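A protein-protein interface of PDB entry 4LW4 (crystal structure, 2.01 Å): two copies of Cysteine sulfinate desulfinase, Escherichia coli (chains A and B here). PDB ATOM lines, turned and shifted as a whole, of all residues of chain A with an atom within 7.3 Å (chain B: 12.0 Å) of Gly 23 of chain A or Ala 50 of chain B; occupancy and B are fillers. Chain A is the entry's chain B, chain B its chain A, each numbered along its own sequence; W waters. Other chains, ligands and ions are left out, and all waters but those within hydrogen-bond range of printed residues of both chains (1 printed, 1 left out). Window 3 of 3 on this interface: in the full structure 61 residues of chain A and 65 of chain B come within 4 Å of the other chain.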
ATOM      1  N   ARG A  13      10.251 -16.395 -32.672  1.00  0.00           N
ATOM      2  CA  ARG A  13      10.487 -16.208 -31.256  1.00  0.00           C
ATOM      3  C   ARG A  13       9.292 -15.619 -30.502  1.00  0.00           C
ATOM      4  O   ARG A  13       8.973 -16.026 -29.438  1.00  0.00           O
ATOM      5  CB  ARG A  13      11.767 -15.422 -31.006  1.00  0.00           C
ATOM      6  CG  ARG A  13      12.040 -15.123 -29.592  1.00  0.00           C
ATOM      7  CD  ARG A  13      13.374 -14.441 -29.366  1.00  0.00           C
ATOM      8  NE  ARG A  13      13.524 -14.050 -27.988  1.00  0.00           N
ATOM      9  CZ  ARG A  13      14.252 -14.666 -27.063  1.00  0.00           C
ATOM     10  NH1 ARG A  13      14.959 -15.753 -27.310  1.00  0.00           N
ATOM     11  NH2 ARG A  13      14.277 -14.170 -25.852  1.00  0.00           N
ATOM     12  N   PRO A  17       5.423 -17.998 -25.318  1.00  0.00           N
ATOM     13  CA  PRO A  17       5.192 -17.246 -24.062  1.00  0.00           C
ATOM     14  C   PRO A  17       6.294 -17.454 -23.077  1.00  0.00           C
ATOM     15  O   PRO A  17       6.536 -16.573 -22.290  1.00  0.00           O
ATOM     16  CB  PRO A  17       3.887 -17.860 -23.489  1.00  0.00           C
ATOM     17  CG  PRO A  17       3.727 -19.226 -24.293  1.00  0.00           C
ATOM     18  CD  PRO A  17       4.278 -18.884 -25.640  1.00  0.00           C
ATOM     19  N   ALA A  18       6.968 -18.618 -23.085  1.00  0.00           N
ATOM     20  CA  ALA A  18       8.045 -18.850 -22.116  1.00  0.00           C
ATOM     21  C   ALA A  18       9.232 -17.881 -22.262  1.00  0.00           C
ATOM     22  O   ALA A  18      10.043 -17.748 -21.371  1.00  0.00           O
ATOM     23  CB  ALA A  18       8.534 -20.307 -22.199  1.00  0.00           C
ATOM     24  N   LEU A  19       9.360 -17.255 -23.424  1.00  0.00           N
ATOM     25  CA  LEU A  19      10.488 -16.347 -23.713  1.00  0.00           C
ATOM     26  C   LEU A  19      10.119 -14.863 -23.519  1.00  0.00           C
ATOM     27  O   LEU A  19      10.971 -13.981 -23.688  1.00  0.00           O
ATOM     28  CB  LEU A  19      10.985 -16.559 -25.165  1.00  0.00           C
ATOM     29  CG  LEU A  19      11.668 -17.922 -25.377  1.00  0.00           C
ATOM     30  CD1 LEU A  19      12.067 -18.122 -26.803  1.00  0.00           C
ATOM     31  CD2 LEU A  19      12.875 -18.072 -24.428  1.00  0.00           C
ATOM     32  N   GLN A  20       8.887 -14.586 -23.137  1.00  0.00           N
ATOM     33  CA  GLN A  20       8.482 -13.217 -22.952  1.00  0.00           C
ATOM     34  C   GLN A  20       9.324 -12.521 -21.878  1.00  0.00           C
ATOM     35  O   GLN A  20       9.723 -11.413 -22.049  1.00  0.00           O
ATOM     36  CB  GLN A  20       6.961 -13.089 -22.774  1.00  0.00           C
ATOM     37  CG  GLN A  20       6.199 -13.121 -24.129  1.00  0.00           C
ATOM     38  CD  GLN A  20       4.684 -13.134 -23.976  1.00  0.00           C
ATOM     39  OE1 GLN A  20       4.144 -12.629 -23.001  1.00  0.00           O
ATOM     40  NE2 GLN A  20       4.003 -13.700 -24.935  1.00  0.00           N
ATOM     41  N   ASP A  21       9.656 -13.195 -20.807  1.00  0.00           N
ATOM     42  CA  ASP A  21      10.546 -12.611 -19.860  1.00  0.00           C
ATOM     43  C   ASP A  21      11.824 -13.360 -19.735  1.00  0.00           C
ATOM     44  O   ASP A  21      11.901 -14.570 -19.862  1.00  0.00           O
ATOM     45  CB  ASP A  21       9.920 -12.499 -18.505  1.00  0.00           C
ATOM     46  CG  ASP A  21       9.274 -11.193 -18.303  1.00  0.00           C
ATOM     47  OD1 ASP A  21       9.866 -10.359 -17.608  1.00  0.00           O
ATOM     48  OD2 ASP A  21       8.191 -10.979 -18.845  1.00  0.00           O
ATOM     49  N   ALA A  22      12.819 -12.594 -19.417  1.00  0.00           N
ATOM     50  CA  ALA A  22      14.189 -13.026 -19.395  1.00  0.00           C
ATOM     51  C   ALA A  22      14.379 -14.497 -19.060  1.00  0.00           C
ATOM     52  O   ALA A  22      13.590 -15.158 -18.421  1.00  0.00           O
ATOM     53  CB  ALA A  22      14.986 -12.146 -18.468  1.00  0.00           C
ATOM     54  N   GLY A  23      15.450 -14.984 -19.605  1.00  0.00           N
ATOM     55  CA  GLY A  23      15.934 -16.308 -19.443  1.00  0.00           C
ATOM     56  C   GLY A  23      16.545 -16.624 -20.783  1.00  0.00           C
ATOM     57  O   GLY A  23      16.030 -16.270 -21.791  1.00  0.00           O
ATOM     58  N   VAL A  24      17.633 -17.350 -20.750  1.00  0.00           N
ATOM     59  CA  VAL A  24      18.225 -17.839 -21.937  1.00  0.00           C
ATOM     60  C   VAL A  24      18.052 -19.320 -21.882  1.00  0.00           C
ATOM     61  O   VAL A  24      18.596 -19.949 -21.029  1.00  0.00           O
ATOM     62  CB  VAL A  24      19.700 -17.504 -22.003  1.00  0.00           C
ATOM     63  CG1 VAL A  24      20.342 -18.195 -23.110  1.00  0.00           C
ATOM     64  CG2 VAL A  24      19.897 -16.013 -22.119  1.00  0.00           C
ATOM     65  N   TYR A  25      17.325 -19.850 -22.833  1.00  0.00           N
ATOM     66  CA  TYR A  25      17.017 -21.311 -22.866  1.00  0.00           C
ATOM     67  C   TYR A  25      17.829 -21.985 -23.969  1.00  0.00           C
ATOM     68  O   TYR A  25      17.640 -21.680 -25.141  1.00  0.00           O
ATOM     69  CB  TYR A  25      15.527 -21.534 -23.126  1.00  0.00           C
ATOM     70  CG  TYR A  25      15.123 -22.988 -22.979  1.00  0.00           C
ATOM     71  CD1 TYR A  25      15.003 -23.552 -21.701  1.00  0.00           C
ATOM     72  CD2 TYR A  25      14.945 -23.806 -24.099  1.00  0.00           C
ATOM     73  CE1 TYR A  25      14.682 -24.908 -21.522  1.00  0.00           C
ATOM     74  CE2 TYR A  25      14.610 -25.213 -23.950  1.00  0.00           C
ATOM     75  CZ  TYR A  25      14.464 -25.749 -22.667  1.00  0.00           C
ATOM     76  OH  TYR A  25      14.105 -27.107 -22.461  1.00  0.00           O
ATOM     77  N   LEU A  26      18.736 -22.861 -23.582  1.00  0.00           N
ATOM     78  CA  LEU A  26      19.592 -23.570 -24.522  1.00  0.00           C
ATOM     79  C   LEU A  26      19.601 -25.032 -24.275  1.00  0.00           C
ATOM     80  O   LEU A  26      20.648 -25.658 -24.358  1.00  0.00           O
ATOM     81  CB  LEU A  26      21.051 -23.026 -24.484  1.00  0.00           C
ATOM     82  CG  LEU A  26      21.211 -21.575 -24.988  1.00  0.00           C
ATOM     83  CD1 LEU A  26      22.637 -21.011 -24.610  1.00  0.00           C
ATOM     84  CD2 LEU A  26      20.879 -21.500 -26.522  1.00  0.00           C
ATOM     85  N   LEU A  33      10.599 -25.518 -26.042  1.00  0.00           N
ATOM     86  CA  LEU A  33       9.553 -24.586 -25.578  1.00  0.00           C
ATOM     87  C   LEU A  33       8.332 -24.723 -26.486  1.00  0.00           C
ATOM     88  O   LEU A  33       8.432 -25.244 -27.628  1.00  0.00           O
ATOM     89  CB  LEU A  33      10.063 -23.149 -25.528  1.00  0.00           C
ATOM     90  CG  LEU A  33      11.362 -22.993 -24.699  1.00  0.00           C
ATOM     91  CD1 LEU A  33      11.748 -21.486 -24.684  1.00  0.00           C
ATOM     92  CD2 LEU A  33      11.153 -23.493 -23.280  1.00  0.00           C
ATOM     93  N   GLY A 352      21.529 -17.613 -15.266  1.00  0.00           N
ATOM     94  CA  GLY A 352      20.345 -17.499 -16.141  1.00  0.00           C
ATOM     95  C   GLY A 352      20.443 -18.140 -17.520  1.00  0.00           C
ATOM     96  O   GLY A 352      19.667 -17.800 -18.419  1.00  0.00           O
ATOM     97  N   ILE A 353      21.344 -19.099 -17.660  1.00  0.00           N
ATOM     98  CA  ILE A 353      21.471 -19.931 -18.876  1.00  0.00           C
ATOM     99  C   ILE A 353      21.060 -21.391 -18.538  1.00  0.00           C
ATOM    100  O   ILE A 353      21.695 -22.063 -17.703  1.00  0.00           O
ATOM    101  CB  ILE A 353      22.944 -19.989 -19.448  1.00  0.00           C
ATOM    102  CG1 ILE A 353      23.671 -18.632 -19.404  1.00  0.00           C
ATOM    103  CG2 ILE A 353      22.961 -20.542 -20.873  1.00  0.00           C
ATOM    104  CD1 ILE A 353      22.925 -17.400 -19.941  1.00  0.00           C
ATOM    105  N   ALA A 354      20.027 -21.887 -19.212  1.00  0.00           N
ATOM    106  CA  ALA A 354      19.604 -23.256 -19.027  1.00  0.00           C
ATOM    107  C   ALA A 354      20.257 -24.173 -20.093  1.00  0.00           C
ATOM    108  O   ALA A 354      19.963 -24.073 -21.309  1.00  0.00           O
ATOM    109  CB  ALA A 354      18.064 -23.326 -19.033  1.00  0.00           C
ATOM    110  N   ASN A 383      16.008 -18.915 -30.500  1.00  0.00           N
ATOM    111  CA  ASN A 383      17.228 -18.386 -29.916  1.00  0.00           C
ATOM    112  C   ASN A 383      17.761 -17.238 -30.730  1.00  0.00           C
ATOM    113  O   ASN A 383      17.398 -17.022 -31.900  1.00  0.00           O
ATOM    114  CB  ASN A 383      18.300 -19.505 -29.742  1.00  0.00           C
ATOM    115  CG  ASN A 383      17.949 -20.441 -28.570  1.00  0.00           C
ATOM    116  OD1 ASN A 383      17.807 -21.647 -28.740  1.00  0.00           O
ATOM    117  ND2 ASN A 383      17.741 -19.851 -27.358  1.00  0.00           N
ATOM    118  N   ASP A 387      21.427 -14.459 -26.940  1.00  0.00           N
ATOM    119  CA  ASP A 387      21.648 -15.761 -26.271  1.00  0.00           C
ATOM    120  C   ASP A 387      23.098 -16.238 -26.341  1.00  0.00           C
ATOM    121  O   ASP A 387      23.652 -16.724 -25.346  1.00  0.00           O
ATOM    122  CB  ASP A 387      20.690 -16.852 -26.823  1.00  0.00           C
ATOM    123  CG  ASP A 387      19.221 -16.520 -26.537  1.00  0.00           C
ATOM    124  OD1 ASP A 387      18.919 -15.685 -25.614  1.00  0.00           O
ATOM    125  OD2 ASP A 387      18.349 -17.080 -27.193  1.00  0.00           O
ATOM    126  N   GLN B  43      -1.521 -24.952 -18.139  1.00  0.00           N
ATOM    127  CA  GLN B  43      -1.233 -23.671 -18.789  1.00  0.00           C
ATOM    128  C   GLN B  43       0.084 -23.135 -18.288  1.00  0.00           C
ATOM    129  O   GLN B  43       0.940 -22.757 -19.082  1.00  0.00           O
ATOM    130  CB  GLN B  43      -2.375 -22.668 -18.497  1.00  0.00           C
ATOM    131  CG  GLN B  43      -1.970 -21.161 -18.783  1.00  0.00           C
ATOM    132  CD  GLN B  43      -2.381 -20.724 -20.172  1.00  0.00           C
ATOM    133  OE1 GLN B  43      -3.329 -21.249 -20.729  1.00  0.00           O
ATOM    134  NE2 GLN B  43      -1.668 -19.766 -20.742  1.00  0.00           N
ATOM    135  N   GLN B  44       0.270 -23.193 -16.969  1.00  0.00           N
ATOM    136  CA  GLN B  44       1.483 -22.713 -16.339  1.00  0.00           C
ATOM    137  C   GLN B  44       2.717 -23.498 -16.728  1.00  0.00           C
ATOM    138  O   GLN B  44       3.761 -22.901 -16.955  1.00  0.00           O
ATOM    139  CB  GLN B  44       1.346 -22.773 -14.825  1.00  0.00           C
ATOM    140  CG  GLN B  44       0.355 -21.729 -14.301  1.00  0.00           C
ATOM    141  CD  GLN B  44       0.229 -21.850 -12.797  1.00  0.00           C
ATOM    142  OE1 GLN B  44      -0.276 -22.858 -12.266  1.00  0.00           O
ATOM    143  NE2 GLN B  44       0.736 -20.851 -12.090  1.00  0.00           N
ATOM    144  N   PHE B  45       2.572 -24.818 -16.802  1.00  0.00           N
ATOM    145  CA  PHE B  45       3.685 -25.706 -17.141  1.00  0.00           C
ATOM    146  C   PHE B  45       4.169 -25.453 -18.607  1.00  0.00           C
ATOM    147  O   PHE B  45       5.350 -25.202 -18.859  1.00  0.00           O
ATOM    148  CB  PHE B  45       3.265 -27.170 -16.993  1.00  0.00           C
ATOM    149  CG  PHE B  45       4.328 -28.127 -17.490  1.00  0.00           C
ATOM    150  CD1 PHE B  45       5.546 -28.250 -16.786  1.00  0.00           C
ATOM    151  CD2 PHE B  45       4.135 -28.845 -18.677  1.00  0.00           C
ATOM    152  CE1 PHE B  45       6.563 -29.071 -17.242  1.00  0.00           C
ATOM    153  CE2 PHE B  45       5.107 -29.671 -19.186  1.00  0.00           C
ATOM    154  CZ  PHE B  45       6.366 -29.812 -18.491  1.00  0.00           C
ATOM    155  N   TYR B  46       3.237 -25.371 -19.542  1.00  0.00           N
ATOM    156  CA  TYR B  46       3.649 -25.167 -20.953  1.00  0.00           C
ATOM    157  C   TYR B  46       4.002 -23.746 -21.278  1.00  0.00           C
ATOM    158  O   TYR B  46       4.485 -23.453 -22.378  1.00  0.00           O
ATOM    159  CB  TYR B  46       2.524 -25.611 -21.857  1.00  0.00           C
ATOM    160  CG  TYR B  46       2.374 -27.120 -21.960  1.00  0.00           C
ATOM    161  CD1 TYR B  46       3.509 -27.978 -22.192  1.00  0.00           C
ATOM    162  CD2 TYR B  46       1.133 -27.692 -21.881  1.00  0.00           C
ATOM    163  CE1 TYR B  46       3.342 -29.379 -22.338  1.00  0.00           C
ATOM    164  CE2 TYR B  46       0.945 -29.116 -22.036  1.00  0.00           C
ATOM    165  CZ  TYR B  46       2.055 -29.913 -22.275  1.00  0.00           C
ATOM    166  OH  TYR B  46       1.853 -31.277 -22.432  1.00  0.00           O
ATOM    167  N   SER B  47       3.732 -22.836 -20.346  1.00  0.00           N
ATOM    168  CA  SER B  47       4.070 -21.435 -20.532  1.00  0.00           C
ATOM    169  C   SER B  47       5.259 -20.985 -19.739  1.00  0.00           C
ATOM    170  O   SER B  47       5.528 -19.822 -19.750  1.00  0.00           O
ATOM    171  CB  SER B  47       2.901 -20.524 -20.079  1.00  0.00           C
ATOM    172  OG  SER B  47       1.875 -20.800 -20.975  1.00  0.00           O
ATOM    173  N   LEU B  48       5.939 -21.864 -19.049  1.00  0.00           N
ATOM    174  CA  LEU B  48       6.806 -21.447 -17.950  1.00  0.00           C
ATOM    175  C   LEU B  48       8.070 -20.725 -18.436  1.00  0.00           C
ATOM    176  O   LEU B  48       8.877 -21.286 -19.210  1.00  0.00           O
ATOM    177  CB  LEU B  48       7.200 -22.641 -17.054  1.00  0.00           C
ATOM    178  CG  LEU B  48       8.099 -22.420 -15.820  1.00  0.00           C
ATOM    179  CD1 LEU B  48       7.301 -21.809 -14.610  1.00  0.00           C
ATOM    180  CD2 LEU B  48       8.844 -23.685 -15.387  1.00  0.00           C
ATOM    181  N   SER B  49       8.257 -19.508 -17.890  1.00  0.00           N
ATOM    182  CA  SER B  49       9.404 -18.639 -18.201  1.00  0.00           C
ATOM    183  C   SER B  49      10.701 -19.392 -18.273  1.00  0.00           C
ATOM    184  O   SER B  49      11.118 -19.999 -17.293  1.00  0.00           O
ATOM    185  CB  SER B  49       9.525 -17.449 -17.205  1.00  0.00           C
ATOM    186  OG  SER B  49       8.688 -16.400 -17.673  1.00  0.00           O
ATOM    187  N   ALA B  50      11.308 -19.327 -19.456  1.00  0.00           N
ATOM    188  CA  ALA B  50      12.570 -19.995 -19.812  1.00  0.00           C
ATOM    189  C   ALA B  50      13.687 -19.581 -18.923  1.00  0.00           C
ATOM    190  O   ALA B  50      13.910 -18.373 -18.740  1.00  0.00           O
ATOM    191  CB  ALA B  50      12.944 -19.647 -21.224  1.00  0.00           C
ATOM    192  N   GLY B  51      14.412 -20.583 -18.418  1.00  0.00           N
ATOM    193  CA  GLY B  51      15.394 -20.403 -17.346  1.00  0.00           C
ATOM    194  C   GLY B  51      14.643 -20.374 -16.025  1.00  0.00           C
ATOM    195  O   GLY B  51      14.981 -19.607 -15.130  1.00  0.00           O
ATOM    196  N   PHE B  58      10.035 -17.333 -10.971  1.00  0.00           N
ATOM    197  CA  PHE B  58      10.570 -18.317 -10.024  1.00  0.00           C
ATOM    198  C   PHE B  58       9.539 -18.844  -8.998  1.00  0.00           C
ATOM    199  O   PHE B  58       9.751 -19.912  -8.401  1.00  0.00           O
ATOM    200  CB  PHE B  58      11.837 -17.796  -9.313  1.00  0.00           C
ATOM    201  CG  PHE B  58      12.580 -18.862  -8.537  1.00  0.00           C
ATOM    202  CD1 PHE B  58      12.398 -18.999  -7.154  1.00  0.00           C
ATOM    203  CD2 PHE B  58      13.449 -19.749  -9.195  1.00  0.00           C
ATOM    204  CE1 PHE B  58      13.081 -20.007  -6.426  1.00  0.00           C
ATOM    205  CE2 PHE B  58      14.137 -20.757  -8.489  1.00  0.00           C
ATOM    206  CZ  PHE B  58      13.954 -20.889  -7.098  1.00  0.00           C
ATOM    207  N   ALA B  59       8.444 -18.101  -8.797  1.00  0.00           N
ATOM    208  CA  ALA B  59       7.349 -18.519  -7.895  1.00  0.00           C
ATOM    209  C   ALA B  59       6.331 -19.509  -8.541  1.00  0.00           C
ATOM    210  O   ALA B  59       5.853 -20.445  -7.891  1.00  0.00           O
ATOM    211  CB  ALA B  59       6.634 -17.290  -7.313  1.00  0.00           C
ATOM    212  N   GLU B  60       5.984 -19.297  -9.808  1.00  0.00           N
ATOM    213  CA  GLU B  60       5.221 -20.308 -10.554  1.00  0.00           C
ATOM    214  C   GLU B  60       6.095 -21.559 -10.739  1.00  0.00           C
ATOM    215  O   GLU B  60       5.621 -22.683 -10.493  1.00  0.00           O
ATOM    216  CB  GLU B  60       4.728 -19.781 -11.912  1.00  0.00           C
ATOM    217  CG  GLU B  60       3.432 -18.972 -11.857  1.00  0.00           C
ATOM    218  CD  GLU B  60       2.807 -18.720 -13.241  1.00  0.00           C
ATOM    219  OE1 GLU B  60       2.838 -19.633 -14.116  1.00  0.00           O
ATOM    220  OE2 GLU B  60       2.257 -17.605 -13.443  1.00  0.00           O
ATOM    221  N   ALA B  61       7.363 -21.348 -11.133  1.00  0.00           N
ATOM    222  CA  ALA B  61       8.356 -22.412 -11.287  1.00  0.00           C
ATOM    223  C   ALA B  61       8.401 -23.337 -10.077  1.00  0.00           C
ATOM    224  O   ALA B  61       8.288 -24.555 -10.225  1.00  0.00           O
ATOM    225  CB  ALA B  61       9.743 -21.834 -11.565  1.00  0.00           C
ATOM    226  N   GLN B  62       8.556 -22.752  -8.882  1.00  0.00           N
ATOM    227  CA  GLN B  62       8.664 -23.536  -7.657  1.00  0.00           C
ATOM    228  C   GLN B  62       7.371 -24.277  -7.304  1.00  0.00           C
ATOM    229  O   GLN B  62       7.436 -25.418  -6.897  1.00  0.00           O
ATOM    230  CB  GLN B  62       9.168 -22.679  -6.499  1.00  0.00           C
ATOM    231  CG  GLN B  62      10.557 -23.117  -6.019  1.00  0.00           C
ATOM    232  CD  GLN B  62      10.505 -24.015  -4.757  1.00  0.00           C
ATOM    233  OE1 GLN B  62       9.710 -24.986  -4.674  1.00  0.00           O
ATOM    234  NE2 GLN B  62      11.365 -23.692  -3.769  1.00  0.00           N
ATOM    235  N   LEU B  64       5.152 -25.358  -9.486  1.00  0.00           N
ATOM    236  CA  LEU B  64       5.095 -26.523 -10.411  1.00  0.00           C
ATOM    237  C   LEU B  64       6.072 -27.638  -9.986  1.00  0.00           C
ATOM    238  O   LEU B  64       5.720 -28.837  -9.963  1.00  0.00           O
ATOM    239  CB  LEU B  64       5.362 -26.098 -11.861  1.00  0.00           C
ATOM    240  CG  LEU B  64       4.299 -25.200 -12.508  1.00  0.00           C
ATOM    241  CD1 LEU B  64       4.908 -24.570 -13.734  1.00  0.00           C
ATOM    242  CD2 LEU B  64       3.042 -25.967 -12.920  1.00  0.00           C
HETATM  243  O   HOH W   1       8.071 -15.346 -20.030  1.00  0.00           O
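O of Ala 22 of chain A lies close to O of Ala 50 of chain B (3.2 Å).
The backbone NH (N) of Ala 50 of chain B lies within hydrogen-bond range of the backbone carbonyl oxygen (O) of Ala 18 of chain A (2.8 Å).
Of the 17 printed residues of chain A, 5 touch a printed residue of chain B.
Printed residues of chain A that touch a printed residue of chain B: Ala 18, Leu 19, Ala 22, Gly 23 and Tyr 25.
Hydrophobic or aromatic side chains of chain B within 4 Å of the printed part of chain A: Ala 50.
Among the printed residues, 8 pairs touch across the chains.
Among the printed residues, no Asp or Glu carboxylate lies within 4 Å of a Lys or Arg side-chain nitrogen of the other chain.
Ala 18 of chain A touches Ser 47 of chain B (CA to O, 3.6 Å).
Ala 18 of chain A touches Leu 48 of chain B.
Ser 49 of chain B touches Ala 18 of chain A.
CD2 of Leu 19 of chain A touches CB of Ala 50 of chain B, 3.6 Å away.
Gly 23 of chain A touches Ala 50 of chain B.
CB of Ala 50 of chain B touches CB of Tyr 25 of chain A, 3.7 Å away.
Water W1 lies within hydrogen-bond range of OG of Ser 49 of chain B (2.7 Å), N of Asp 21 of chain A (2.8 Å), O of Pro 17 of chain A (3.0 Å), N of Gln 20 of chain A (3.3 Å) and O of Ala 18 of chain A (3.4 Å).
No position is printed for both chains.
Of chain B, only Ala 50 comes within 4 Å of Leu 19 of chain A.
Ala 22 of chain A touches just one residue of chain B: Ala 50.
Gly 23 of chain A touches just one residue of chain B: Ala 50.
Of the printed residues of chain A, Ser 47 of chain B touches Ala 18 (3.6 Å).
Printed residues of chain A within 4 Å of Leu 48 of chain B: Ala 18.
Of the printed residues of chain A, Ser 49 of chain B touches Ala 18.
Of the printed residues of chain A, Ala 50 of chain B touches Ala 18, Leu 19, Ala 22, Gly 23 and Tyr 25.
The nearest residue of chain B that does not touch Gly 23 of chain A is Gly 51 of chain B (4.6 Å).
The nearest printed residue of chain A that does not touch Ser 47 of chain B is Pro 17 of chain A (4.1 Å).
The backbone carbonyl oxygen of Gln 43 of chain B sits at hydrogen-bond distance from the side-chain hydroxyl of Ser 47 of chain B.
ND2 of Asn 383 of chain A is in hydrogen-bond range of O of Tyr 25 of chain A, 2.9 Å away.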
